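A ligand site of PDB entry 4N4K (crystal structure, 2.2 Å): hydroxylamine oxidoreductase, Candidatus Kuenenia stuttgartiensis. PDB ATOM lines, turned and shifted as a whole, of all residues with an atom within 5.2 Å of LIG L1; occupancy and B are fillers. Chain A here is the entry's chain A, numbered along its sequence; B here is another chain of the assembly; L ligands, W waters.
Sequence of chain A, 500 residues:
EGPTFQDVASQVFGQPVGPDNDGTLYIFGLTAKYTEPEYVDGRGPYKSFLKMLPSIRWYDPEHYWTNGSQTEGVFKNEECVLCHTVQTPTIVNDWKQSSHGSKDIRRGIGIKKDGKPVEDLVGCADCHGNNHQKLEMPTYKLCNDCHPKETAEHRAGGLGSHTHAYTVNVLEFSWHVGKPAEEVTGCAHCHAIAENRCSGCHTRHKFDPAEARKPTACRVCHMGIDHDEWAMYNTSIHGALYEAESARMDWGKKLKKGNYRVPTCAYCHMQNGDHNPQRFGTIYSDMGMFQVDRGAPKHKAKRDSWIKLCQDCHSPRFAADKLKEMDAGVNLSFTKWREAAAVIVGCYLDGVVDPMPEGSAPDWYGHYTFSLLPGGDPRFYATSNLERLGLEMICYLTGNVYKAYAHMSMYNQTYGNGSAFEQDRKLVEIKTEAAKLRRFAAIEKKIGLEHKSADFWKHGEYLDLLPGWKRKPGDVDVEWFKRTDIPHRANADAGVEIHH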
ATOM      1  N   TRP A  58      24.429 -12.187 -11.428  1.00  0.00           N
ATOM      2  CA  TRP A  58      24.933 -13.384 -12.111  1.00  0.00           C
ATOM      3  C   TRP A  58      26.152 -13.989 -11.409  1.00  0.00           C
ATOM      4  O   TRP A  58      26.389 -15.193 -11.506  1.00  0.00           O
ATOM      5  CB  TRP A  58      25.308 -13.063 -13.565  1.00  0.00           C
ATOM      6  CG  TRP A  58      24.173 -12.475 -14.361  1.00  0.00           C
ATOM      7  CD1 TRP A  58      23.921 -11.157 -14.571  1.00  0.00           C
ATOM      8  CD2 TRP A  58      23.142 -13.204 -15.034  1.00  0.00           C
ATOM      9  NE1 TRP A  58      22.787 -11.014 -15.336  1.00  0.00           N
ATOM     10  CE2 TRP A  58      22.275 -12.254 -15.611  1.00  0.00           C
ATOM     11  CE3 TRP A  58      22.885 -14.559 -15.222  1.00  0.00           C
ATOM     12  CZ2 TRP A  58      21.148 -12.626 -16.329  1.00  0.00           C
ATOM     13  CZ3 TRP A  58      21.745 -14.922 -15.922  1.00  0.00           C
ATOM     14  CH2 TRP A  58      20.865 -13.956 -16.423  1.00  0.00           C
ATOM     15  N   TRP A  65      20.471 -12.862  -6.768  1.00  0.00           N
ATOM     16  CA  TRP A  65      19.652 -13.413  -7.842  1.00  0.00           C
ATOM     17  C   TRP A  65      18.156 -13.302  -7.544  1.00  0.00           C
ATOM     18  O   TRP A  65      17.712 -13.681  -6.461  1.00  0.00           O
ATOM     19  CB  TRP A  65      20.008 -14.877  -8.105  1.00  0.00           C
ATOM     20  CG  TRP A  65      19.254 -15.471  -9.246  1.00  0.00           C
ATOM     21  CD1 TRP A  65      18.228 -16.377  -9.169  1.00  0.00           C
ATOM     22  CD2 TRP A  65      19.384 -15.123 -10.631  1.00  0.00           C
ATOM     23  NE1 TRP A  65      17.770 -16.677 -10.436  1.00  0.00           N
ATOM     24  CE2 TRP A  65      18.433 -15.891 -11.347  1.00  0.00           C
ATOM     25  CE3 TRP A  65      20.189 -14.227 -11.335  1.00  0.00           C
ATOM     26  CZ2 TRP A  65      18.368 -15.881 -12.740  1.00  0.00           C
ATOM     27  CZ3 TRP A  65      20.105 -14.195 -12.720  1.00  0.00           C
ATOM     28  CH2 TRP A  65      19.169 -14.988 -13.407  1.00  0.00           C
ATOM     29  N   GLY A  68      13.687 -12.847 -13.165  1.00  0.00           N
ATOM     30  CA  GLY A  68      13.556 -11.757 -14.139  1.00  0.00           C
ATOM     31  C   GLY A  68      13.098 -12.252 -15.500  1.00  0.00           C
ATOM     32  O   GLY A  68      13.291 -11.568 -16.508  1.00  0.00           O
ATOM     33  N   SER A  69      12.433 -13.406 -15.509  1.00  0.00           N
ATOM     34  CA  SER A  69      11.954 -14.021 -16.738  1.00  0.00           C
ATOM     35  C   SER A  69      10.523 -13.608 -17.038  1.00  0.00           C
ATOM     36  O   SER A  69       9.760 -13.241 -16.127  1.00  0.00           O
ATOM     37  CB  SER A  69      12.040 -15.552 -16.626  1.00  0.00           C
ATOM     38  OG  SER A  69      11.597 -16.183 -17.805  1.00  0.00           O
ATOM     39  N   GLN A  70      10.187 -13.580 -18.322  1.00  0.00           N
ATOM     40  CA  GLN A  70       8.830 -13.277 -18.780  1.00  0.00           C
ATOM     41  C   GLN A  70       8.088 -14.555 -19.183  1.00  0.00           C
ATOM     42  O   GLN A  70       6.890 -14.502 -19.482  1.00  0.00           O
ATOM     43  CB  GLN A  70       8.865 -12.295 -19.965  1.00  0.00           C
ATOM     44  CG  GLN A  70       9.379 -10.890 -19.619  1.00  0.00           C
ATOM     45  CD  GLN A  70      10.883 -10.842 -19.336  1.00  0.00           C
ATOM     46  OE1 GLN A  70      11.312 -10.329 -18.310  1.00  0.00           O
ATOM     47  NE2 GLN A  70      11.677 -11.468 -20.210  1.00  0.00           N
ATOM     48  N   THR A  71       8.805 -15.663 -19.291  1.00  0.00           N
ATOM     49  CA  THR A  71       8.227 -16.950 -19.661  1.00  0.00           C
ATOM     50  C   THR A  71       7.735 -17.688 -18.414  1.00  0.00           C
ATOM     51  O   THR A  71       8.426 -17.713 -17.394  1.00  0.00           O
ATOM     52  CB  THR A  71       9.254 -17.816 -20.421  1.00  0.00           C
ATOM     53  OG1 THR A  71       9.688 -17.128 -21.593  1.00  0.00           O
ATOM     54  CG2 THR A  71       8.657 -19.164 -20.818  1.00  0.00           C
ATOM     55  N   PHE A  75       8.215 -26.982 -16.456  1.00  0.00           N
ATOM     56  CA  PHE A  75       8.563 -27.815 -17.604  1.00  0.00           C
ATOM     57  C   PHE A  75       9.429 -29.001 -17.232  1.00  0.00           C
ATOM     58  O   PHE A  75      10.125 -28.984 -16.208  1.00  0.00           O
ATOM     59  CB  PHE A  75       9.290 -26.980 -18.651  1.00  0.00           C
ATOM     60  CG  PHE A  75       8.524 -25.782 -19.118  1.00  0.00           C
ATOM     61  CD1 PHE A  75       7.479 -25.918 -20.029  1.00  0.00           C
ATOM     62  CD2 PHE A  75       8.871 -24.505 -18.694  1.00  0.00           C
ATOM     63  CE1 PHE A  75       6.803 -24.805 -20.503  1.00  0.00           C
ATOM     64  CE2 PHE A  75       8.193 -23.390 -19.144  1.00  0.00           C
ATOM     65  CZ  PHE A  75       7.122 -23.545 -20.026  1.00  0.00           C
ATOM     66  N   LYS A  76       9.480 -29.967 -18.145  1.00  0.00           N
ATOM     67  CA  LYS A  76      10.393 -31.098 -18.039  1.00  0.00           C
ATOM     68  C   LYS A  76      11.621 -30.838 -18.924  1.00  0.00           C
ATOM     69  O   LYS A  76      11.563 -30.001 -19.817  1.00  0.00           O
ATOM     70  CB  LYS A  76       9.692 -32.391 -18.453  1.00  0.00           C
ATOM     71  CG  LYS A  76      10.471 -33.662 -18.124  1.00  0.00           C
ATOM     72  CD  LYS A  76      10.692 -33.871 -16.611  1.00  0.00           C
ATOM     73  CE  LYS A  76      12.153 -34.174 -16.284  1.00  0.00           C
ATOM     74  NZ  LYS A  76      12.628 -35.378 -17.019  1.00  0.00           N
ATOM     75  N   GLU A  79      11.427 -30.403 -22.573  1.00  0.00           N
ATOM     76  CA  GLU A  79      10.755 -29.176 -22.981  1.00  0.00           C
ATOM     77  C   GLU A  79      11.693 -27.957 -22.929  1.00  0.00           C
ATOM     78  O   GLU A  79      11.625 -27.088 -23.785  1.00  0.00           O
ATOM     79  CB  GLU A  79       9.495 -28.935 -22.127  1.00  0.00           C
ATOM     80  CG  GLU A  79       8.421 -30.000 -22.317  1.00  0.00           C
ATOM     81  CD  GLU A  79       7.231 -29.869 -21.374  1.00  0.00           C
ATOM     82  OE1 GLU A  79       6.134 -30.323 -21.763  1.00  0.00           O
ATOM     83  OE2 GLU A  79       7.418 -29.510 -20.188  1.00  0.00           O
ATOM     84  N   CYS A  80      12.595 -27.942 -21.943  1.00  0.00           N
ATOM     85  CA  CYS A  80      13.653 -26.921 -21.891  1.00  0.00           C
ATOM     86  C   CYS A  80      14.460 -26.919 -23.186  1.00  0.00           C
ATOM     87  O   CYS A  80      14.553 -25.899 -23.862  1.00  0.00           O
ATOM     88  CB  CYS A  80      14.631 -27.163 -20.732  1.00  0.00           C
ATOM     89  SG  CYS A  80      13.914 -27.417 -19.099  1.00  0.00           S
ATOM     90  N   CYS A  83      12.514 -25.779 -26.669  1.00  0.00           N
ATOM     91  CA  CYS A  83      12.260 -24.353 -26.809  1.00  0.00           C
ATOM     92  C   CYS A  83      13.569 -23.568 -26.909  1.00  0.00           C
ATOM     93  O   CYS A  83      13.731 -22.736 -27.801  1.00  0.00           O
ATOM     94  CB  CYS A  83      11.419 -23.816 -25.653  1.00  0.00           C
ATOM     95  SG  CYS A  83      10.898 -22.096 -25.872  1.00  0.00           S
ATOM     96  N   HIS A  84      14.557 -23.933 -26.090  1.00  0.00           N
ATOM     97  CA  HIS A  84      15.851 -23.254 -26.121  1.00  0.00           C
ATOM     98  C   HIS A  84      16.655 -23.568 -27.377  1.00  0.00           C
ATOM     99  O   HIS A  84      17.530 -22.795 -27.734  1.00  0.00           O
ATOM    100  CB  HIS A  84      16.664 -23.564 -24.859  1.00  0.00           C
ATOM    101  CG  HIS A  84      16.303 -22.694 -23.696  1.00  0.00           C
ATOM    102  ND1 HIS A  84      16.765 -21.396 -23.586  1.00  0.00           N
ATOM    103  CD2 HIS A  84      15.312 -22.806 -22.781  1.00  0.00           C
ATOM    104  CE1 HIS A  84      16.108 -20.780 -22.627  1.00  0.00           C
ATOM    105  NE2 HIS A  84      15.255 -21.626 -22.099  1.00  0.00           N
ATOM    106  N   GLN A  87      15.385 -20.587 -28.894  1.00  0.00           N
ATOM    107  CA  GLN A  87      15.598 -19.303 -28.207  1.00  0.00           C
ATOM    108  C   GLN A  87      17.064 -18.974 -27.889  1.00  0.00           C
ATOM    109  O   GLN A  87      17.418 -17.798 -27.841  1.00  0.00           O
ATOM    110  CB  GLN A  87      14.734 -19.232 -26.946  1.00  0.00           C
ATOM    111  CG  GLN A  87      13.249 -19.074 -27.230  1.00  0.00           C
ATOM    112  CD  GLN A  87      12.929 -17.781 -27.968  1.00  0.00           C
ATOM    113  OE1 GLN A  87      13.445 -16.712 -27.628  1.00  0.00           O
ATOM    114  NE2 GLN A  87      12.091 -17.878 -28.992  1.00  0.00           N
ATOM    115  N   CYS A 124      18.710 -29.095 -18.334  1.00  0.00           N
ATOM    116  CA  CYS A 124      18.546 -27.698 -17.930  1.00  0.00           C
ATOM    117  C   CYS A 124      17.852 -27.571 -16.577  1.00  0.00           C
ATOM    118  O   CYS A 124      18.208 -26.714 -15.771  1.00  0.00           O
ATOM    119  CB  CYS A 124      17.721 -26.944 -18.984  1.00  0.00           C
ATOM    120  SG  CYS A 124      18.056 -27.353 -20.722  1.00  0.00           S
ATOM    121  N   ALA A 125      16.813 -28.371 -16.377  1.00  0.00           N
ATOM    122  CA  ALA A 125      15.978 -28.292 -15.181  1.00  0.00           C
ATOM    123  C   ALA A 125      16.717 -28.805 -13.944  1.00  0.00           C
ATOM    124  O   ALA A 125      16.508 -28.283 -12.850  1.00  0.00           O
ATOM    125  CB  ALA A 125      14.667 -29.062 -15.384  1.00  0.00           C
ATOM    126  N   HIS A 128      18.925 -25.725 -13.168  1.00  0.00           N
ATOM    127  CA  HIS A 128      18.281 -24.412 -13.080  1.00  0.00           C
ATOM    128  C   HIS A 128      16.905 -24.415 -12.419  1.00  0.00           C
ATOM    129  O   HIS A 128      16.344 -23.346 -12.176  1.00  0.00           O
ATOM    130  CB  HIS A 128      18.163 -23.805 -14.480  1.00  0.00           C
ATOM    131  CG  HIS A 128      19.472 -23.410 -15.067  1.00  0.00           C
ATOM    132  ND1 HIS A 128      20.192 -22.319 -14.617  1.00  0.00           N
ATOM    133  CD2 HIS A 128      20.170 -23.901 -16.122  1.00  0.00           C
ATOM    134  CE1 HIS A 128      21.297 -22.203 -15.319  1.00  0.00           C
ATOM    135  NE2 HIS A 128      21.313 -23.155 -16.237  1.00  0.00           N
ATOM    136  N   GLY A 129      16.331 -25.600 -12.210  1.00  0.00           N
ATOM    137  CA  GLY A 129      14.970 -25.726 -11.695  1.00  0.00           C
ATOM    138  C   GLY A 129      13.970 -25.964 -12.818  1.00  0.00           C
ATOM    139  O   GLY A 129      14.236 -25.639 -13.977  1.00  0.00           O
ATOM    140  N   ASN A 130      12.747 -26.310 -12.426  1.00  0.00           N
ATOM    141  CA  ASN A 130      11.679 -26.690 -13.353  1.00  0.00           C
ATOM    142  C   ASN A 130      10.726 -25.546 -13.658  1.00  0.00           C
ATOM    143  O   ASN A 130       9.938 -25.648 -14.595  1.00  0.00           O
ATOM    144  CB  ASN A 130      10.872 -27.861 -12.754  1.00  0.00           C
ATOM    145  CG  ASN A 130      11.658 -29.161 -12.740  1.00  0.00           C
ATOM    146  OD1 ASN A 130      11.677 -29.888 -13.745  1.00  0.00           O
ATOM    147  ND2 ASN A 130      12.098 -29.583 -11.550  1.00  0.00           N
ATOM    148  N   HIS A 132       9.830 -21.820 -14.540  1.00  0.00           N
ATOM    149  CA  HIS A 132      10.486 -20.769 -15.304  1.00  0.00           C
ATOM    150  C   HIS A 132      10.396 -19.397 -14.626  1.00  0.00           C
ATOM    151  O   HIS A 132      11.033 -18.447 -15.087  1.00  0.00           O
ATOM    152  CB  HIS A 132       9.918 -20.682 -16.728  1.00  0.00           C
ATOM    153  CG  HIS A 132      10.936 -20.276 -17.752  1.00  0.00           C
ATOM    154  ND1 HIS A 132      11.411 -18.995 -17.858  1.00  0.00           N
ATOM    155  CD2 HIS A 132      11.683 -21.034 -18.595  1.00  0.00           C
ATOM    156  CE1 HIS A 132      12.364 -18.955 -18.776  1.00  0.00           C
ATOM    157  NE2 HIS A 132      12.573 -20.183 -19.203  1.00  0.00           N
ATOM    158  N   LEU A 135      13.619 -19.701 -11.671  1.00  0.00           N
ATOM    159  CA  LEU A 135      14.842 -20.272 -12.231  1.00  0.00           C
ATOM    160  C   LEU A 135      16.023 -19.936 -11.330  1.00  0.00           C
ATOM    161  O   LEU A 135      16.028 -18.899 -10.668  1.00  0.00           O
ATOM    162  CB  LEU A 135      15.099 -19.749 -13.653  1.00  0.00           C
ATOM    163  CG  LEU A 135      14.140 -20.287 -14.717  1.00  0.00           C
ATOM    164  CD1 LEU A 135      14.300 -19.509 -16.020  1.00  0.00           C
ATOM    165  CD2 LEU A 135      14.347 -21.783 -14.937  1.00  0.00           C
ATOM    166  N   GLU A 136      16.955 -20.875 -11.224  1.00  0.00           N
ATOM    167  CA  GLU A 136      18.107 -20.747 -10.339  1.00  0.00           C
ATOM    168  C   GLU A 136      19.397 -20.497 -11.130  1.00  0.00           C
ATOM    169  O   GLU A 136      19.526 -20.966 -12.253  1.00  0.00           O
ATOM    170  CB  GLU A 136      18.247 -22.015  -9.488  1.00  0.00           C
ATOM    171  CG  GLU A 136      17.135 -22.170  -8.440  1.00  0.00           C
ATOM    172  CD  GLU A 136      16.863 -23.616  -8.049  1.00  0.00           C
ATOM    173  OE1 GLU A 136      15.768 -23.876  -7.486  1.00  0.00           O
ATOM    174  OE2 GLU A 136      17.731 -24.487  -8.274  1.00  0.00           O
ATOM    175  N   MET A 137      20.247 -19.623 -10.601  1.00  0.00           N
ATOM    176  CA  MET A 137      21.541 -19.350 -11.189  1.00  0.00           C
ATOM    177  C   MET A 137      22.608 -19.905 -10.230  1.00  0.00           C
ATOM    178  O   MET A 137      22.787 -19.386  -9.129  1.00  0.00           O
ATOM    179  CB  MET A 137      21.704 -17.837 -11.419  1.00  0.00           C
ATOM    180  CG  MET A 137      22.699 -17.459 -12.496  1.00  0.00           C
ATOM    181  SD  MET A 137      22.488 -18.352 -14.057  1.00  0.00           S
ATOM    182  CE  MET A 137      20.789 -18.017 -14.459  1.00  0.00           C
ATOM    183  N   GLN B 311      21.608 -13.200 -27.911  1.00  0.00           N
ATOM    184  CA  GLN B 311      20.672 -14.274 -27.575  1.00  0.00           C
ATOM    185  C   GLN B 311      20.830 -15.513 -28.459  1.00  0.00           C
ATOM    186  O   GLN B 311      20.266 -16.556 -28.134  1.00  0.00           O
ATOM    187  CB  GLN B 311      19.219 -13.779 -27.593  1.00  0.00           C
ATOM    188  CG  GLN B 311      18.259 -14.642 -26.780  1.00  0.00           C
ATOM    189  CD  GLN B 311      16.799 -14.249 -26.944  1.00  0.00           C
ATOM    190  OE1 GLN B 311      16.467 -13.058 -26.953  1.00  0.00           O
ATOM    191  NE2 GLN B 311      15.917 -15.236 -26.906  1.00  0.00           N
ATOM    192  N   SER B 315      21.108 -15.810 -22.446  1.00  0.00           N
ATOM    193  CA  SER B 315      19.893 -15.172 -21.979  1.00  0.00           C
ATOM    194  C   SER B 315      19.912 -13.711 -22.399  1.00  0.00           C
ATOM    195  O   SER B 315      20.952 -13.056 -22.245  1.00  0.00           O
ATOM    196  CB  SER B 315      19.809 -15.247 -20.456  1.00  0.00           C
ATOM    197  OG  SER B 315      19.021 -14.186 -19.940  1.00  0.00           O
ATOM    198  N   PRO B 316      18.756 -13.159 -22.817  1.00  0.00           N
ATOM    199  CA  PRO B 316      18.723 -11.740 -23.167  1.00  0.00           C
ATOM    200  C   PRO B 316      18.872 -10.796 -21.960  1.00  0.00           C
ATOM    201  O   PRO B 316      19.218  -9.638 -22.138  1.00  0.00           O
ATOM    202  CB  PRO B 316      17.343 -11.582 -23.837  1.00  0.00           C
ATOM    203  CG  PRO B 316      16.518 -12.669 -23.250  1.00  0.00           C
ATOM    204  CD  PRO B 316      17.454 -13.814 -23.017  1.00  0.00           C
ATOM    205  N   ARG B 317      18.481 -11.285 -20.790  1.00  0.00           N
ATOM    206  CA  ARG B 317      18.641 -10.570 -19.528  1.00  0.00           C
ATOM    207  C   ARG B 317      20.117 -10.363 -19.224  1.00  0.00           C
ATOM    208  O   ARG B 317      20.546  -9.275 -18.837  1.00  0.00           O
ATOM    209  CB  ARG B 317      17.989 -11.381 -18.411  1.00  0.00           C
ATOM    210  CG  ARG B 317      17.906 -10.675 -17.088  1.00  0.00           C
ATOM    211  CD  ARG B 317      17.343 -11.606 -16.032  1.00  0.00           C
ATOM    212  NE  ARG B 317      17.195 -10.941 -14.747  1.00  0.00           N
ATOM    213  CZ  ARG B 317      16.994 -11.560 -13.602  1.00  0.00           C
ATOM    214  NH1 ARG B 317      16.868 -12.882 -13.579  1.00  0.00           N
ATOM    215  NH2 ARG B 317      16.860 -10.863 -12.481  1.00  0.00           N
ATOM    216  N   PHE B 318      20.905 -11.417 -19.427  1.00  0.00           N
ATOM    217  CA  PHE B 318      22.361 -11.402 -19.240  1.00  0.00           C
ATOM    218  C   PHE B 318      23.027 -10.439 -20.220  1.00  0.00           C
ATOM    219  O   PHE B 318      23.802  -9.567 -19.821  1.00  0.00           O
ATOM    220  CB  PHE B 318      22.940 -12.804 -19.419  1.00  0.00           C
ATOM    221  CG  PHE B 318      24.433 -12.862 -19.314  1.00  0.00           C
ATOM    222  CD1 PHE B 318      25.072 -12.547 -18.119  1.00  0.00           C
ATOM    223  CD2 PHE B 318      25.207 -13.235 -20.405  1.00  0.00           C
ATOM    224  CE1 PHE B 318      26.451 -12.539 -18.049  1.00  0.00           C
ATOM    225  CE2 PHE B 318      26.586 -13.289 -20.316  1.00  0.00           C
ATOM    226  CZ  PHE B 318      27.207 -12.989 -19.120  1.00  0.00           C
HETATM  227 FE1  LIG L   1      13.942 -20.875 -20.648  1.00  0.00          FE
HETATM  228  C1  LIG L   1      15.483 -17.839 -20.502  1.00  0.00           C
HETATM  229  C2  LIG L   1      16.000 -22.034 -18.146  1.00  0.00           C
HETATM  230  C3  LIG L   1      12.309 -23.893 -20.684  1.00  0.00           C
HETATM  231  C4  LIG L   1      11.900 -19.785 -23.186  1.00  0.00           C
HETATM  232  N1  LIG L   1      15.530 -20.113 -19.604  1.00  0.00           N
HETATM  233  C5  LIG L   1      15.884 -18.790 -19.586  1.00  0.00           C
HETATM  234  C6  LIG L   1      16.960 -18.628 -18.637  1.00  0.00           C
HETATM  235  C7  LIG L   1      17.128 -19.783 -17.991  1.00  0.00           C
HETATM  236  C8  LIG L   1      16.229 -20.752 -18.596  1.00  0.00           C
HETATM  237  C9  LIG L   1      18.248 -20.102 -16.964  1.00  0.00           C
HETATM  238  C10 LIG L   1      17.580 -17.288 -18.241  1.00  0.00           C
HETATM  239  C11 LIG L   1      16.612 -16.636 -17.245  1.00  0.00           C
HETATM  240  C12 LIG L   1      17.017 -15.220 -16.919  1.00  0.00           C
HETATM  241  O1  LIG L   1      17.525 -14.514 -17.822  1.00  0.00           O
HETATM  242  O2  LIG L   1      16.719 -14.760 -15.790  1.00  0.00           O
HETATM  243  N2  LIG L   1      14.120 -22.610 -19.588  1.00  0.00           N
HETATM  244  C13 LIG L   1      15.099 -22.922 -18.678  1.00  0.00           C
HETATM  245  C14 LIG L   1      14.805 -24.238 -18.139  1.00  0.00           C
HETATM  246  C15 LIG L   1      13.770 -24.733 -18.827  1.00  0.00           C
HETATM  247  C16 LIG L   1      13.375 -23.753 -19.809  1.00  0.00           C
HETATM  248  C17 LIG L   1      15.588 -24.955 -17.019  1.00  0.00           C
HETATM  249  C18 LIG L   1      12.991 -26.007 -18.511  1.00  0.00           C
HETATM  250  C19 LIG L   1      12.609 -26.265 -17.247  1.00  0.00           C
HETATM  251  N3  LIG L   1      12.360 -21.659 -21.692  1.00  0.00           N
HETATM  252  C20 LIG L   1      11.884 -22.954 -21.585  1.00  0.00           C
HETATM  253  C21 LIG L   1      10.763 -23.105 -22.486  1.00  0.00           C
HETATM  254  C22 LIG L   1      10.685 -21.988 -23.226  1.00  0.00           C
HETATM  255  C23 LIG L   1      11.668 -21.050 -22.713  1.00  0.00           C
HETATM  256  C24 LIG L   1       9.947 -24.393 -22.659  1.00  0.00           C
HETATM  257  C25 LIG L   1       9.802 -21.755 -24.474  1.00  0.00           C
HETATM  258  C26 LIG L   1       8.569 -22.284 -24.565  1.00  0.00           C
HETATM  259  N4  LIG L   1      13.745 -19.105 -21.701  1.00  0.00           N
HETATM  260  C27 LIG L   1      12.798 -18.872 -22.690  1.00  0.00           C
HETATM  261  C28 LIG L   1      12.987 -17.551 -23.227  1.00  0.00           C
HETATM  262  C29 LIG L   1      14.035 -16.903 -22.332  1.00  0.00           C
HETATM  263  C30 LIG L   1      14.429 -17.937 -21.390  1.00  0.00           C
HETATM  264  C31 LIG L   1      12.106 -16.841 -24.289  1.00  0.00           C
HETATM  265  C32 LIG L   1      14.532 -15.446 -22.389  1.00  0.00           C
HETATM  266  C33 LIG L   1      13.395 -14.471 -22.102  1.00  0.00           C
HETATM  267  C34 LIG L   1      12.747 -14.774 -20.771  1.00  0.00           C
HETATM  268  O3  LIG L   1      11.494 -14.904 -20.737  1.00  0.00           O
HETATM  269  O4  LIG L   1      13.485 -14.841 -19.750  1.00  0.00           O
HETATM  270 FE1  LG2 L   2      22.796 -23.358 -17.714  1.00  0.00          FE
HETATM  271  C1  LG2 L   2      23.837 -20.259 -16.669  1.00  0.00           C
HETATM  272  C2  LG2 L   2      20.560 -21.939 -19.853  1.00  0.00           C
HETATM  273  C3  LG2 L   2      21.752 -26.473 -18.720  1.00  0.00           C
HETATM  274  C4  LG2 L   2      24.767 -24.850 -15.319  1.00  0.00           C
HETATM  275  N1  LG2 L   2      22.358 -21.472 -18.233  1.00  0.00           N
HETATM  276  C5  LG2 L   2      22.885 -20.327 -17.666  1.00  0.00           C
HETATM  277  C6  LG2 L   2      22.298 -19.195 -18.357  1.00  0.00           C
HETATM  278  C7  LG2 L   2      21.369 -19.656 -19.191  1.00  0.00           C
HETATM  279  C8  LG2 L   2      21.356 -21.098 -19.103  1.00  0.00           C
HETATM  280  C9  LG2 L   2      20.441 -18.815 -20.091  1.00  0.00           C
HETATM  281  C10 LG2 L   2      22.606 -17.713 -18.063  1.00  0.00           C
HETATM  282  C11 LG2 L   2      24.007 -17.337 -18.574  1.00  0.00           C
HETATM  283  C12 LG2 L   2      24.043 -17.253 -20.082  1.00  0.00           C
HETATM  284  O1  LG2 L   2      25.129 -17.550 -20.665  1.00  0.00           O
HETATM  285  O2  LG2 L   2      23.131 -16.616 -20.652  1.00  0.00           O
HETATM  286  N2  LG2 L   2      21.414 -24.067 -19.058  1.00  0.00           N
HETATM  287  C13 LG2 L   2      20.517 -23.311 -19.768  1.00  0.00           C
HETATM  288  C14 LG2 L   2      19.755 -24.207 -20.624  1.00  0.00           C
HETATM  289  C15 LG2 L   2      20.178 -25.443 -20.395  1.00  0.00           C
HETATM  290  C16 LG2 L   2      21.145 -25.394 -19.312  1.00  0.00           C
HETATM  291  C17 LG2 L   2      18.694 -23.804 -21.672  1.00  0.00           C
HETATM  292  C18 LG2 L   2      19.689 -26.719 -21.108  1.00  0.00           C
HETATM  293  C19 LG2 L   2      19.864 -26.832 -22.428  1.00  0.00           C
HETATM  294  N3  LG2 L   2      23.208 -25.288 -17.139  1.00  0.00           N
HETATM  295  C20 LG2 L   2      22.649 -26.424 -17.689  1.00  0.00           C
HETATM  296  C21 LG2 L   2      23.176 -27.575 -16.973  1.00  0.00           C
HETATM  297  C22 LG2 L   2      23.966 -27.135 -15.996  1.00  0.00           C
HETATM  298  C23 LG2 L   2      23.939 -25.674 -16.041  1.00  0.00           C
HETATM  299  C24 LG2 L   2      22.848 -29.047 -17.302  1.00  0.00           C
HETATM  300  C25 LG2 L   2      24.492 -27.992 -14.827  1.00  0.00           C
HETATM  301  C26 LG2 L   2      25.244 -29.079 -15.062  1.00  0.00           C
HETATM  302  N4  LG2 L   2      24.196 -22.661 -16.297  1.00  0.00           N
HETATM  303  C27 LG2 L   2      24.856 -23.484 -15.395  1.00  0.00           C
HETATM  304  C28 LG2 L   2      25.702 -22.674 -14.554  1.00  0.00           C
HETATM  305  C29 LG2 L   2      25.350 -21.224 -14.909  1.00  0.00           C
HETATM  306  C30 LG2 L   2      24.446 -21.321 -16.046  1.00  0.00           C
HETATM  307  C31 LG2 L   2      26.654 -23.141 -13.435  1.00  0.00           C
HETATM  308  C32 LG2 L   2      25.908 -19.947 -14.259  1.00  0.00           C
HETATM  309  C33 LG2 L   2      27.093 -19.392 -15.049  1.00  0.00           C
HETATM  310  C34 LG2 L   2      28.323 -20.233 -14.860  1.00  0.00           C
HETATM  311  O3  LG2 L   2      29.153 -20.284 -15.813  1.00  0.00           O
HETATM  312  O4  LG2 L   2      28.583 -20.691 -13.723  1.00  0.00           O
HETATM  313  O   HOH W   1      15.651 -13.705 -19.656  1.00  0.00           O
HETATM  314  O   HOH W   2      14.693 -15.347 -13.960  1.00  0.00           O
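The side-chain sulfur (SG) of Cys 83 is bonded to a carbon (C25) of LIG L1, 1.8 Å away. C18 of LG2 L2 is bonded to SG of Cys 124, at 1.8 Å. A ring nitrogen (NE2) of His 84 binds an iron atom (FE1) of LIG L1 (2.1 Å). The backbone NH of Thr 71 lies within hydrogen-bond range of an oxygen (O3) of LIG L1 (3.1 Å). A ring nitrogen (NE2) of His 132 binds an iron atom (FE1) of LIG L1 (2.1 Å). An oxygen (O3) of LIG L1 sits at hydrogen-bond distance from the side-chain hydroxyl (OG1) of Thr 71. The backbone NH of Ser 315 of chain B lies within hydrogen-bond range of an oxygen (O2) of LG2 L2, 2.8 Å away. NE2 of His 128 binds FE1 of LG2 L2 (2.1 Å). NE2 of Gln 70 lies within hydrogen-bond range of O3 of LIG L1 (3.5 Å). The side-chain hydroxyl (OG) of Ser 69 sits at hydrogen-bond distance from an oxygen (O4) of LIG L1 (3.0 Å). C18 of LIG L1 is covalently linked to SG of Cys 80, 1.8 Å away. The guanidinium group of Arg 317 of chain B is in salt-bridge range of an oxygen (O2) of LIG L1, 2.9 Å away. O1 of LIG L1 lies within hydrogen-bond range of OG of Ser 315 of chain B (2.6 Å). N of Gln 70 is in hydrogen-bond range of O3 of LIG L1 (3.0 Å).
The backbone carbonyl oxygen of Gly 68 sits close to the side-chain amide oxygen of Gln 70 (2.9 Å). The side-chain hydroxyl (OG) of Ser 315 of chain B sits at hydrogen-bond distance from the backbone NH (N) of Arg 317 of chain B (3.1 Å). The backbone NH (N) of Thr 71 sits at hydrogen-bond distance from the side-chain hydroxyl (OG) of Ser 69 (3.2 Å). The backbone carbonyl oxygen (O) of Asn 130 is in hydrogen-bond range of the backbone NH (N) of Phe 75, at 2.9 Å. ND1 of His 132 sits at hydrogen-bond distance from O of Thr 71. The side-chain amide oxygen (OE1) of Gln 87 sits at hydrogen-bond distance from the side-chain amide nitrogen (NE2) of Gln 311 of chain B, 3.0 Å away. The side-chain hydroxyl (OG) of Ser 69 is in hydrogen-bond range of a ring nitrogen (ND1) of His 132 (2.8 Å). The side-chain hydroxyl (OG) of Ser 315 of chain B lies within hydrogen-bond range of the backbone NH (N) of Phe 318 of chain B (3.4 Å).
Residues that only touch LIG L1: Glu 79 (3.4 Å), Cys 124 (3.4 Å), Gly 129 (3.4 Å), Pro 316 of chain B (3.4 Å), Trp 65 (3.4 Å), Leu 135 (3.4 Å), Gln 87 (3.6 Å), Trp 58 (3.7 Å), Phe 75 (3.7 Å), Ala 125 (3.7 Å), His 128 (3.8 Å) and Asn 130 (3.8 Å). Within 4 Å of LIG L1: Trp 58, Trp 65, Ser 69, Gln 70, Thr 71, Phe 75, Glu 79, Cys 80, Cys 83, His 84, Gln 87, Cys 124, Ala 125, His 128, Gly 129, Asn 130, His 132, Leu 135, Ser 315 of chain B, Pro 316 of chain B and Arg 317 of chain B. The nearest printed residue that does not touch LIG L1 is Met 137 (4.1 Å).
Water W1 bridges O4 of LIG L1 (2.4 Å) and OG of Ser 315 of chain B (3.4 Å).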
